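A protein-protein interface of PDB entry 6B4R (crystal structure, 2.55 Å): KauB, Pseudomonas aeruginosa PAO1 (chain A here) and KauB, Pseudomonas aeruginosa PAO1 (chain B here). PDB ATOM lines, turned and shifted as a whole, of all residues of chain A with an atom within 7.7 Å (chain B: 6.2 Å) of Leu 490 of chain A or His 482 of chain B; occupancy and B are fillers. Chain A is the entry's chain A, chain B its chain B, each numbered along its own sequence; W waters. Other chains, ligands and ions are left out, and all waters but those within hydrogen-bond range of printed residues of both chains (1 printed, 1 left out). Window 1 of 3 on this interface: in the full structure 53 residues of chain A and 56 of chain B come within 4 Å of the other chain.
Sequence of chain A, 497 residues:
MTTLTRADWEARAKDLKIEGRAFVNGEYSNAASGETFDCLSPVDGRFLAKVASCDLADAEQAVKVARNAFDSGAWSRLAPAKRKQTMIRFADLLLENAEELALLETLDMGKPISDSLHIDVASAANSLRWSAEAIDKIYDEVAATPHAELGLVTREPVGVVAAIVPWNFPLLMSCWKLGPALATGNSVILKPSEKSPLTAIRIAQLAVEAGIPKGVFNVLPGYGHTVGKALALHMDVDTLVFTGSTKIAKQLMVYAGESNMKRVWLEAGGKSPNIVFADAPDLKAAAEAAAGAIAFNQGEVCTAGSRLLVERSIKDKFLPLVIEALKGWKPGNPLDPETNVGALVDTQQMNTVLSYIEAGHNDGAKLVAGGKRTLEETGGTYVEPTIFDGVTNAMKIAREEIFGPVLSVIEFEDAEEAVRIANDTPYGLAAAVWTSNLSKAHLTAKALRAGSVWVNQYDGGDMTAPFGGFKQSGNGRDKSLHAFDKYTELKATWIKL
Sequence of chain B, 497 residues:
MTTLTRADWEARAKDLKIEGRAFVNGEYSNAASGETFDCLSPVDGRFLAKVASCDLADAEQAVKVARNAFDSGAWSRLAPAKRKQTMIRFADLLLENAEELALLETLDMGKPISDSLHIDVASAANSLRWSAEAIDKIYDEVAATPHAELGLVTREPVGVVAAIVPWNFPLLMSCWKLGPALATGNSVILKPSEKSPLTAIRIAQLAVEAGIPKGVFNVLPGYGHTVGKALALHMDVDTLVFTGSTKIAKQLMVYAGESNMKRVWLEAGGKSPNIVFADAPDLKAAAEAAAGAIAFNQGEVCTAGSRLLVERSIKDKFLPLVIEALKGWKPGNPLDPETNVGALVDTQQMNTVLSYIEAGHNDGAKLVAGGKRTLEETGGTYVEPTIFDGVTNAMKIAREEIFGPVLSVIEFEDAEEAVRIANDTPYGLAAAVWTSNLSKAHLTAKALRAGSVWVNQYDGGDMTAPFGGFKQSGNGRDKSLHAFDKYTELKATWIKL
Hydrophobic or aromatic side chains of chain A within 4 Å of the printed part of chain B: Val 153, Leu 490 and Ala 492. Of the 16 printed residues of chain B, 7 touch a printed residue of chain A. Hydrophobic or aromatic side chains of chain B that line the printed part of chain A: Pro 466, Phe 470 and His 482.
The backbone carbonyl oxygen of Glu 141 of chain A lies within hydrogen-bond range of the backbone NH of Val 153 of chain A (2.9 Å). The guanidinium group (NH2) of Arg 263 of chain A lies within salt-bridge range of the side-chain carboxylate (OE1) of Glu 489 of chain A. The backbone carbonyl oxygen of Thr 154 of chain A is in hydrogen-bond range of the backbone NH of Lys 491 of chain A, 2.8 Å away. OG of Ser 480 of chain B sits at hydrogen-bond distance from N of His 482 of chain B (3.2 Å). The backbone NH (N) of Glu 489 of chain A sits at hydrogen-bond distance from the backbone carbonyl oxygen (O) of Glu 156 of chain A, at 2.7 Å. The side-chain carboxylate of Glu 156 of chain A is in salt-bridge range of the side-chain amino group of Lys 491 of chain A.
Val 153 of chain A touches Pro 466 of chain B (CG1 to CG, 3.6 Å). Glu 156 of chain A touches Phe 470 of chain B (OE2 to CE2, 3.7 Å). Arg 263 of chain A touches Phe 470 of chain B. Glu 489 of chain A touches Phe 470 of chain B. O of Leu 490 of chain A touches CE1 of Phe 470 of chain B, at 3.5 Å. His 482 of chain B touches Leu 490 of chain A (CG to CD1, 3.7 Å). Ala 450 of chain B touches Lys 491 of chain A. Lys 491 of chain A touches Gly 451 of chain B (CA to O, 3.3 Å). CA of Ser 452 of chain B touches O of Ala 492 of chain A, 3.5 Å away. Ala 492 of chain A touches Pro 466 of chain B (CB to O, 3.4 Å).
Leu 490 of chain A touches just these residues of chain B: Gly 451, Phe 470, Arg 477 and His 482. Of chain A, only Glu 141 (3.0 Å) and Leu 490 (3.7 Å) come within 4 Å of His 482 of chain B. Printed residues of chain B within 4 Å of Glu 141 of chain A: His 482 (3.0 Å). Of the printed residues of chain A, Gly 451 of chain B touches Leu 490, Lys 491 and Ala 492. Printed residues of chain A within 4 Å of Ala 450 of chain B: Lys 491 (3.4 Å). Printed residues of chain B within 4 Å of Glu 156 of chain A: Phe 470 (3.7 Å). Arg 155 of chain A touches none of the printed residues of chain B. Gly 468 of chain B touches none of the printed residues of chain A. The nearest printed residue of chain A that does not touch His 482 of chain B is Arg 155 of chain A (4.3 Å). The nearest printed residue of chain B that does not touch Arg 263 of chain A is Arg 477 of chain B (5.1 Å).
A ring nitrogen (NE2) of His 482 of chain B lies within hydrogen-bond range of the side-chain carboxylate (OE1) of Glu 141 of chain A, at 3.0 Å. The backbone carbonyl oxygen of Gly 451 of chain B lies within hydrogen-bond range of the backbone NH of Ala 492 of chain A, at 2.7 Å. The side-chain carboxylate of Glu 489 of chain A lies within salt-bridge range of the guanidinium group of Arg 477 of chain B. The guanidinium group (NH2) of Arg 477 of chain B lies within hydrogen-bond range of the backbone carbonyl oxygen (O) of Leu 490 of chain A (2.8 Å).
Water W1 lies within hydrogen-bond range of OE2 of Glu 489 of chain A (2.9 Å), N of Leu 490 of chain A (3.1 Å) and NH2 of Arg 477 of chain B (3.5 Å).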
ATOM      1  N   ASP A 140     -15.432   3.979   3.071  1.00  0.00           N
ATOM      2  CA  ASP A 140     -16.067   5.162   2.499  1.00  0.00           C
ATOM      3  C   ASP A 140     -17.585   4.991   2.499  1.00  0.00           C
ATOM      4  O   ASP A 140     -18.102   4.020   3.045  1.00  0.00           O
ATOM      5  CB  ASP A 140     -15.535   5.453   1.093  1.00  0.00           C
ATOM      6  CG  ASP A 140     -14.103   5.960   1.108  1.00  0.00           C
ATOM      7  OD1 ASP A 140     -13.681   6.516   2.144  1.00  0.00           O
ATOM      8  OD2 ASP A 140     -13.397   5.806   0.087  1.00  0.00           O
ATOM      9  N   GLU A 141     -18.300   5.928   1.884  1.00  0.00           N
ATOM     10  CA  GLU A 141     -19.747   5.990   2.066  1.00  0.00           C
ATOM     11  C   GLU A 141     -20.567   5.759   0.797  1.00  0.00           C
ATOM     12  O   GLU A 141     -20.104   6.010  -0.315  1.00  0.00           O
ATOM     13  CB  GLU A 141     -20.131   7.334   2.695  1.00  0.00           C
ATOM     14  CG  GLU A 141     -19.390   7.640   3.991  1.00  0.00           C
ATOM     15  CD  GLU A 141     -19.542   9.089   4.431  1.00  0.00           C
ATOM     16  OE1 GLU A 141     -19.749   9.964   3.563  1.00  0.00           O
ATOM     17  OE2 GLU A 141     -19.456   9.352   5.648  1.00  0.00           O
ATOM     18  N   LEU A 152     -21.751   7.663  -4.475  1.00  0.00           N
ATOM     19  CA  LEU A 152     -20.562   7.238  -3.754  1.00  0.00           C
ATOM     20  C   LEU A 152     -19.811   8.435  -3.192  1.00  0.00           C
ATOM     21  O   LEU A 152     -19.589   9.426  -3.889  1.00  0.00           O
ATOM     22  CB  LEU A 152     -19.636   6.451  -4.682  1.00  0.00           C
ATOM     23  CG  LEU A 152     -20.253   5.248  -5.396  1.00  0.00           C
ATOM     24  CD1 LEU A 152     -19.231   4.591  -6.311  1.00  0.00           C
ATOM     25  CD2 LEU A 152     -20.795   4.250  -4.383  1.00  0.00           C
ATOM     26  N   VAL A 153     -19.417   8.340  -1.928  1.00  0.00           N
ATOM     27  CA  VAL A 153     -18.596   9.370  -1.314  1.00  0.00           C
ATOM     28  C   VAL A 153     -17.282   8.746  -0.871  1.00  0.00           C
ATOM     29  O   VAL A 153     -17.215   8.093   0.168  1.00  0.00           O
ATOM     30  CB  VAL A 153     -19.300  10.024  -0.112  1.00  0.00           C
ATOM     31  CG1 VAL A 153     -18.444  11.145   0.456  1.00  0.00           C
ATOM     32  CG2 VAL A 153     -20.667  10.550  -0.524  1.00  0.00           C
ATOM     33  N   THR A 154     -16.240   8.946  -1.671  1.00  0.00           N
ATOM     34  CA  THR A 154     -14.960   8.285  -1.447  1.00  0.00           C
ATOM     35  C   THR A 154     -13.837   9.269  -1.137  1.00  0.00           C
ATOM     36  O   THR A 154     -13.959  10.469  -1.392  1.00  0.00           O
ATOM     37  CB  THR A 154     -14.556   7.425  -2.664  1.00  0.00           C
ATOM     38  OG1 THR A 154     -14.566   8.233  -3.849  1.00  0.00           O
ATOM     39  CG2 THR A 154     -15.522   6.262  -2.841  1.00  0.00           C
ATOM     40  N   ARG A 155     -12.744   8.751  -0.582  1.00  0.00           N
ATOM     41  CA  ARG A 155     -11.568   9.561  -0.286  1.00  0.00           C
ATOM     42  C   ARG A 155     -10.393   9.195  -1.188  1.00  0.00           C
ATOM     43  O   ARG A 155     -10.191   8.029  -1.519  1.00  0.00           O
ATOM     44  CB  ARG A 155     -11.169   9.425   1.184  1.00  0.00           C
ATOM     45  CG  ARG A 155     -12.150  10.069   2.143  1.00  0.00           C
ATOM     46  CD  ARG A 155     -11.541  10.235   3.524  1.00  0.00           C
ATOM     47  NE  ARG A 155     -12.397  11.027   4.403  1.00  0.00           N
ATOM     48  CZ  ARG A 155     -12.319  12.347   4.536  1.00  0.00           C
ATOM     49  NH1 ARG A 155     -11.419  13.036   3.844  1.00  0.00           N
ATOM     50  NH2 ARG A 155     -13.141  12.979   5.362  1.00  0.00           N
ATOM     51  N   GLU A 156      -9.625  10.204  -1.587  1.00  0.00           N
ATOM     52  CA  GLU A 156      -8.472  10.000  -2.454  1.00  0.00           C
ATOM     53  C   GLU A 156      -7.295  10.812  -1.945  1.00  0.00           C
ATOM     54  O   GLU A 156      -7.480  11.921  -1.448  1.00  0.00           O
ATOM     55  CB  GLU A 156      -8.799  10.419  -3.887  1.00  0.00           C
ATOM     56  CG  GLU A 156      -9.884   9.596  -4.548  1.00  0.00           C
ATOM     57  CD  GLU A 156     -10.249  10.123  -5.917  1.00  0.00           C
ATOM     58  OE1 GLU A 156     -11.101   9.504  -6.588  1.00  0.00           O
ATOM     59  OE2 GLU A 156      -9.680  11.158  -6.320  1.00  0.00           O
ATOM     60  N   VAL A 158      -4.237  13.327  -1.601  1.00  0.00           N
ATOM     61  CA  VAL A 158      -4.072  14.668  -2.163  1.00  0.00           C
ATOM     62  C   VAL A 158      -2.943  14.744  -3.193  1.00  0.00           C
ATOM     63  O   VAL A 158      -3.030  15.495  -4.165  1.00  0.00           O
ATOM     64  CB  VAL A 158      -3.845  15.730  -1.067  1.00  0.00           C
ATOM     65  CG1 VAL A 158      -5.130  15.987  -0.305  1.00  0.00           C
ATOM     66  CG2 VAL A 158      -2.732  15.299  -0.120  1.00  0.00           C
ATOM     67  N   ARG A 263      -3.811  23.127   1.157  1.00  0.00           N
ATOM     68  CA  ARG A 263      -4.369  22.816   2.468  1.00  0.00           C
ATOM     69  C   ARG A 263      -3.282  22.943   3.522  1.00  0.00           C
ATOM     70  O   ARG A 263      -2.151  22.502   3.316  1.00  0.00           O
ATOM     71  CB  ARG A 263      -4.968  21.407   2.505  1.00  0.00           C
ATOM     72  CG  ARG A 263      -6.259  21.247   1.720  1.00  0.00           C
ATOM     73  CD  ARG A 263      -5.997  20.739   0.312  1.00  0.00           C
ATOM     74  NE  ARG A 263      -7.239  20.546  -0.430  1.00  0.00           N
ATOM     75  CZ  ARG A 263      -7.785  21.463  -1.221  1.00  0.00           C
ATOM     76  NH1 ARG A 263      -7.194  22.641  -1.381  1.00  0.00           N
ATOM     77  NH2 ARG A 263      -8.920  21.200  -1.856  1.00  0.00           N
ATOM     78  N   ASP A 485      -7.762  12.219   7.324  1.00  0.00           N
ATOM     79  CA  ASP A 485      -8.561  13.209   6.606  1.00  0.00           C
ATOM     80  C   ASP A 485      -7.731  14.396   6.124  1.00  0.00           C
ATOM     81  O   ASP A 485      -8.129  15.107   5.201  1.00  0.00           O
ATOM     82  CB  ASP A 485      -9.717  13.706   7.478  1.00  0.00           C
ATOM     83  CG  ASP A 485     -10.683  12.596   7.860  1.00  0.00           C
ATOM     84  OD1 ASP A 485     -10.703  11.552   7.171  1.00  0.00           O
ATOM     85  OD2 ASP A 485     -11.427  12.777   8.848  1.00  0.00           O
ATOM     86  N   THR A 488      -6.384  13.411   2.498  1.00  0.00           N
ATOM     87  CA  THR A 488      -7.315  12.934   1.485  1.00  0.00           C
ATOM     88  C   THR A 488      -8.335  13.997   1.095  1.00  0.00           C
ATOM     89  O   THR A 488      -8.596  14.936   1.850  1.00  0.00           O
ATOM     90  CB  THR A 488      -8.069  11.661   1.932  1.00  0.00           C
ATOM     91  OG1 THR A 488      -8.652  11.869   3.225  1.00  0.00           O
ATOM     92  CG2 THR A 488      -7.129  10.463   1.978  1.00  0.00           C
ATOM     93  N   GLU A 489      -8.898  13.834  -0.097  1.00  0.00           N
ATOM     94  CA  GLU A 489      -9.975  14.687  -0.577  1.00  0.00           C
ATOM     95  C   GLU A 489     -11.253  13.866  -0.702  1.00  0.00           C
ATOM     96  O   GLU A 489     -11.205  12.674  -0.994  1.00  0.00           O
ATOM     97  CB  GLU A 489      -9.619  15.281  -1.941  1.00  0.00           C
ATOM     98  CG  GLU A 489      -8.392  16.173  -1.948  1.00  0.00           C
ATOM     99  CD  GLU A 489      -8.731  17.640  -1.760  1.00  0.00           C
ATOM    100  OE1 GLU A 489      -8.189  18.473  -2.517  1.00  0.00           O
ATOM    101  OE2 GLU A 489      -9.537  17.959  -0.858  1.00  0.00           O
ATOM    102  N   LEU A 490     -12.392  14.509  -0.475  1.00  0.00           N
ATOM    103  CA  LEU A 490     -13.683  13.859  -0.647  1.00  0.00           C
ATOM    104  C   LEU A 490     -14.164  13.979  -2.087  1.00  0.00           C
ATOM    105  O   LEU A 490     -14.068  15.042  -2.700  1.00  0.00           O
ATOM    106  CB  LEU A 490     -14.716  14.477   0.292  1.00  0.00           C
ATOM    107  CG  LEU A 490     -14.614  14.063   1.756  1.00  0.00           C
ATOM    108  CD1 LEU A 490     -15.592  14.860   2.599  1.00  0.00           C
ATOM    109  CD2 LEU A 490     -14.880  12.574   1.890  1.00  0.00           C
ATOM    110  N   LYS A 491     -14.681  12.881  -2.624  1.00  0.00           N
ATOM    111  CA  LYS A 491     -15.235  12.884  -3.970  1.00  0.00           C
ATOM    112  C   LYS A 491     -16.644  12.311  -3.965  1.00  0.00           C
ATOM    113  O   LYS A 491     -16.854  11.168  -3.568  1.00  0.00           O
ATOM    114  CB  LYS A 491     -14.346  12.082  -4.924  1.00  0.00           C
ATOM    115  CG  LYS A 491     -14.987  11.816  -6.276  1.00  0.00           C
ATOM    116  CD  LYS A 491     -14.043  11.083  -7.211  1.00  0.00           C
ATOM    117  CE  LYS A 491     -12.860  11.955  -7.578  1.00  0.00           C
ATOM    118  NZ  LYS A 491     -11.931  11.262  -8.511  1.00  0.00           N
ATOM    119  N   ALA A 492     -17.609  13.112  -4.407  1.00  0.00           N
ATOM    120  CA  ALA A 492     -18.986  12.651  -4.517  1.00  0.00           C
ATOM    121  C   ALA A 492     -19.296  12.215  -5.946  1.00  0.00           C
ATOM    122  O   ALA A 492     -19.512  13.049  -6.826  1.00  0.00           O
ATOM    123  CB  ALA A 492     -19.949  13.734  -4.067  1.00  0.00           C
ATOM    124  N   THR A 493     -19.314  10.904  -6.170  1.00  0.00           N
ATOM    125  CA  THR A 493     -19.618  10.356  -7.486  1.00  0.00           C
ATOM    126  C   THR A 493     -21.084   9.943  -7.588  1.00  0.00           C
ATOM    127  O   THR A 493     -21.480   8.903  -7.064  1.00  0.00           O
ATOM    128  CB  THR A 493     -18.733   9.140  -7.814  1.00  0.00           C
ATOM    129  OG1 THR A 493     -17.353   9.498  -7.684  1.00  0.00           O
ATOM    130  CG2 THR A 493     -18.996   8.659  -9.234  1.00  0.00           C
ATOM    131  N   ALA B 450     -11.802  15.865  -9.148  1.00  0.00           N
ATOM    132  CA  ALA B 450     -12.904  16.786  -8.886  1.00  0.00           C
ATOM    133  C   ALA B 450     -13.710  16.358  -7.664  1.00  0.00           C
ATOM    134  O   ALA B 450     -13.900  15.167  -7.420  1.00  0.00           O
ATOM    135  CB  ALA B 450     -13.804  16.901 -10.107  1.00  0.00           C
ATOM    136  N   GLY B 451     -14.181  17.339  -6.900  1.00  0.00           N
ATOM    137  CA  GLY B 451     -14.958  17.067  -5.705  1.00  0.00           C
ATOM    138  C   GLY B 451     -16.263  16.374  -6.030  1.00  0.00           C
ATOM    139  O   GLY B 451     -16.743  15.534  -5.270  1.00  0.00           O
ATOM    140  N   SER B 452     -16.840  16.733  -7.173  1.00  0.00           N
ATOM    141  CA  SER B 452     -18.066  16.113  -7.646  1.00  0.00           C
ATOM    142  C   SER B 452     -17.851  15.537  -9.038  1.00  0.00           C
ATOM    143  O   SER B 452     -17.318  16.211  -9.916  1.00  0.00           O
ATOM    144  CB  SER B 452     -19.205  17.135  -7.684  1.00  0.00           C
ATOM    145  OG  SER B 452     -19.549  17.580  -6.383  1.00  0.00           O
ATOM    146  N   PRO B 466     -21.711  15.544  -0.557  1.00  0.00           N
ATOM    147  CA  PRO B 466     -20.787  16.622  -0.193  1.00  0.00           C
ATOM    148  C   PRO B 466     -20.337  17.383  -1.440  1.00  0.00           C
ATOM    149  O   PRO B 466     -20.266  16.799  -2.524  1.00  0.00           O
ATOM    150  CB  PRO B 466     -19.613  15.876   0.448  1.00  0.00           C
ATOM    151  CG  PRO B 466     -19.654  14.515  -0.162  1.00  0.00           C
ATOM    152  CD  PRO B 466     -21.112  14.209  -0.375  1.00  0.00           C
ATOM    153  N   GLY B 468     -17.535  20.358  -2.977  1.00  0.00           N
ATOM    154  CA  GLY B 468     -16.327  21.141  -2.805  1.00  0.00           C
ATOM    155  C   GLY B 468     -15.335  20.816  -3.901  1.00  0.00           C
ATOM    156  O   GLY B 468     -15.666  20.093  -4.839  1.00  0.00           O
ATOM    157  N   PHE B 470     -11.067  20.096  -5.445  1.00  0.00           N
ATOM    158  CA  PHE B 470      -9.664  19.739  -5.283  1.00  0.00           C
ATOM    159  C   PHE B 470      -8.836  20.977  -5.611  1.00  0.00           C
ATOM    160  O   PHE B 470      -9.358  21.943  -6.169  1.00  0.00           O
ATOM    161  CB  PHE B 470      -9.258  18.615  -6.244  1.00  0.00           C
ATOM    162  CG  PHE B 470      -9.790  17.252  -5.877  1.00  0.00           C
ATOM    163  CD1 PHE B 470     -10.984  17.100  -5.191  1.00  0.00           C
ATOM    164  CD2 PHE B 470      -9.084  16.114  -6.235  1.00  0.00           C
ATOM    165  CE1 PHE B 470     -11.461  15.842  -4.872  1.00  0.00           C
ATOM    166  CE2 PHE B 470      -9.554  14.856  -5.917  1.00  0.00           C
ATOM    167  CZ  PHE B 470     -10.744  14.719  -5.235  1.00  0.00           C
ATOM    168  N   ARG B 477     -16.085  20.759   2.494  1.00  0.00           N
ATOM    169  CA  ARG B 477     -17.270  20.390   1.735  1.00  0.00           C
ATOM    170  C   ARG B 477     -18.536  21.022   2.316  1.00  0.00           C
ATOM    171  O   ARG B 477     -18.692  21.108   3.534  1.00  0.00           O
ATOM    172  CB  ARG B 477     -17.418  18.862   1.704  1.00  0.00           C
ATOM    173  CG  ARG B 477     -16.276  18.124   1.010  1.00  0.00           C
ATOM    174  CD  ARG B 477     -16.208  18.496  -0.461  1.00  0.00           C
ATOM    175  NE  ARG B 477     -15.147  17.804  -1.190  1.00  0.00           N
ATOM    176  CZ  ARG B 477     -13.940  18.310  -1.418  1.00  0.00           C
ATOM    177  NH1 ARG B 477     -13.625  19.519  -0.969  1.00  0.00           N
ATOM    178  NH2 ARG B 477     -13.045  17.604  -2.099  1.00  0.00           N
ATOM    179  N   ASP B 478     -19.427  21.475   1.438  1.00  0.00           N
ATOM    180  CA  ASP B 478     -20.769  21.883   1.845  1.00  0.00           C
ATOM    181  C   ASP B 478     -21.720  20.704   1.644  1.00  0.00           C
ATOM    182  O   ASP B 478     -21.372  19.733   0.972  1.00  0.00           O
ATOM    183  CB  ASP B 478     -21.250  23.099   1.043  1.00  0.00           C
ATOM    184  CG  ASP B 478     -20.576  24.397   1.473  1.00  0.00           C
ATOM    185  OD1 ASP B 478     -20.469  25.320   0.636  1.00  0.00           O
ATOM    186  OD2 ASP B 478     -20.155  24.502   2.646  1.00  0.00           O
ATOM    187  N   LYS B 479     -22.914  20.796   2.228  1.00  0.00           N
ATOM    188  CA  LYS B 479     -23.902  19.713   2.195  1.00  0.00           C
ATOM    189  C   LYS B 479     -23.408  18.432   2.881  1.00  0.00           C
ATOM    190  O   LYS B 479     -22.303  18.395   3.420  1.00  0.00           O
ATOM    191  CB  LYS B 479     -24.383  19.431   0.763  1.00  0.00           C
ATOM    192  CG  LYS B 479     -25.027  20.634   0.078  1.00  0.00           C
ATOM    193  CD  LYS B 479     -25.718  20.245  -1.221  1.00  0.00           C
ATOM    194  CE  LYS B 479     -24.736  19.669  -2.228  1.00  0.00           C
ATOM    195  NZ  LYS B 479     -25.432  19.102  -3.415  1.00  0.00           N
ATOM    196  N   SER B 480     -24.245  17.394   2.860  1.00  0.00           N
ATOM    197  CA  SER B 480     -23.992  16.135   3.573  1.00  0.00           C
ATOM    198  C   SER B 480     -23.750  16.337   5.073  1.00  0.00           C
ATOM    199  O   SER B 480     -24.059  17.396   5.622  1.00  0.00           O
ATOM    200  CB  SER B 480     -22.850  15.336   2.931  1.00  0.00           C
ATOM    201  OG  SER B 480     -21.589  15.944   3.152  1.00  0.00           O
ATOM    202  N   LEU B 481     -23.214  15.313   5.732  1.00  0.00           N
ATOM    203  CA  LEU B 481     -22.891  15.405   7.154  1.00  0.00           C
ATOM    204  C   LEU B 481     -21.485  15.959   7.352  1.00  0.00           C
ATOM    205  O   LEU B 481     -21.107  16.350   8.460  1.00  0.00           O
ATOM    206  CB  LEU B 481     -22.998  14.034   7.827  1.00  0.00           C
ATOM    207  CG  LEU B 481     -24.361  13.341   7.817  1.00  0.00           C
ATOM    208  CD1 LEU B 481     -24.283  12.022   8.573  1.00  0.00           C
ATOM    209  CD2 LEU B 481     -25.436  14.244   8.405  1.00  0.00           C
ATOM    210  N   HIS B 482     -20.715  15.985   6.270  1.00  0.00           N
ATOM    211  CA  HIS B 482     -19.337  16.455   6.319  1.00  0.00           C
ATOM    212  C   HIS B 482     -19.238  17.969   6.506  1.00  0.00           C
ATOM    213  O   HIS B 482     -18.222  18.472   6.983  1.00  0.00           O
ATOM    214  CB  HIS B 482     -18.576  16.020   5.065  1.00  0.00           C
ATOM    215  CG  HIS B 482     -18.354  14.541   4.979  1.00  0.00           C
ATOM    216  ND1 HIS B 482     -17.349  13.900   5.670  1.00  0.00           N
ATOM    217  CD2 HIS B 482     -19.010  13.580   4.288  1.00  0.00           C
ATOM    218  CE1 HIS B 482     -17.393  12.606   5.406  1.00  0.00           C
ATOM    219  NE2 HIS B 482     -18.392  12.386   4.569  1.00  0.00           N
ATOM    220  N   ALA B 483     -20.294  18.690   6.132  1.00  0.00           N
ATOM    221  CA  ALA B 483     -20.316  20.145   6.278  1.00  0.00           C
ATOM    222  C   ALA B 483     -20.311  20.562   7.744  1.00  0.00           C
ATOM    223  O   ALA B 483     -19.893  21.667   8.080  1.00  0.00           O
ATOM    224  CB  ALA B 483     -21.523  20.736   5.565  1.00  0.00           C
ATOM    225  N   PHE B 484     -20.775  19.668   8.612  1.00  0.00           N
ATOM    226  CA  PHE B 484     -20.840  19.938  10.042  1.00  0.00           C
ATOM    227  C   PHE B 484     -19.454  20.082  10.664  1.00  0.00           C
ATOM    228  O   PHE B 484     -19.278  20.806  11.647  1.00  0.00           O
ATOM    229  CB  PHE B 484     -21.624  18.835  10.758  1.00  0.00           C
ATOM    230  CG  PHE B 484     -23.113  18.917  10.555  1.00  0.00           C
ATOM    231  CD1 PHE B 484     -23.938  19.345  11.580  1.00  0.00           C
ATOM    232  CD2 PHE B 484     -23.685  18.576   9.340  1.00  0.00           C
ATOM    233  CE1 PHE B 484     -25.303  19.428  11.401  1.00  0.00           C
ATOM    234  CE2 PHE B 484     -25.053  18.657   9.156  1.00  0.00           C
ATOM    235  CZ  PHE B 484     -25.862  19.083  10.189  1.00  0.00           C
ATOM    236  N   ASP B 485     -18.473  19.399  10.081  1.00  0.00           N
ATOM    237  CA  ASP B 485     -17.114  19.373  10.623  1.00  0.00           C
ATOM    238  C   ASP B 485     -16.376  20.699  10.455  1.00  0.00           C
ATOM    239  O   ASP B 485     -15.373  20.946  11.125  1.00  0.00           O
ATOM    240  CB  ASP B 485     -16.305  18.241   9.984  1.00  0.00           C
ATOM    241  CG  ASP B 485     -16.908  16.873  10.245  1.00  0.00           C
ATOM    242  OD1 ASP B 485     -17.702  16.746  11.203  1.00  0.00           O
ATOM    243  OD2 ASP B 485     -16.587  15.927   9.495  1.00  0.00           O
ATOM    244  N   LYS B 486     -16.867  21.548   9.560  1.00  0.00           N
ATOM    245  CA  LYS B 486     -16.254  22.853   9.343  1.00  0.00           C
ATOM    246  C   LYS B 486     -16.595  23.830  10.464  1.00  0.00           C
ATOM    247  O   LYS B 486     -15.992  24.897  10.569  1.00  0.00           O
ATOM    248  CB  LYS B 486     -16.687  23.437   7.998  1.00  0.00           C
ATOM    249  CG  LYS B 486     -16.279  22.603   6.799  1.00  0.00           C
ATOM    250  CD  LYS B 486     -16.479  23.365   5.499  1.00  0.00           C
ATOM    251  CE  LYS B 486     -17.931  23.759   5.300  1.00  0.00           C
ATOM    252  NZ  LYS B 486     -18.120  24.528   4.039  1.00  0.00           N
HETATM  253  O   HOH W   1     -11.526  17.084   0.989  1.00  0.00           O
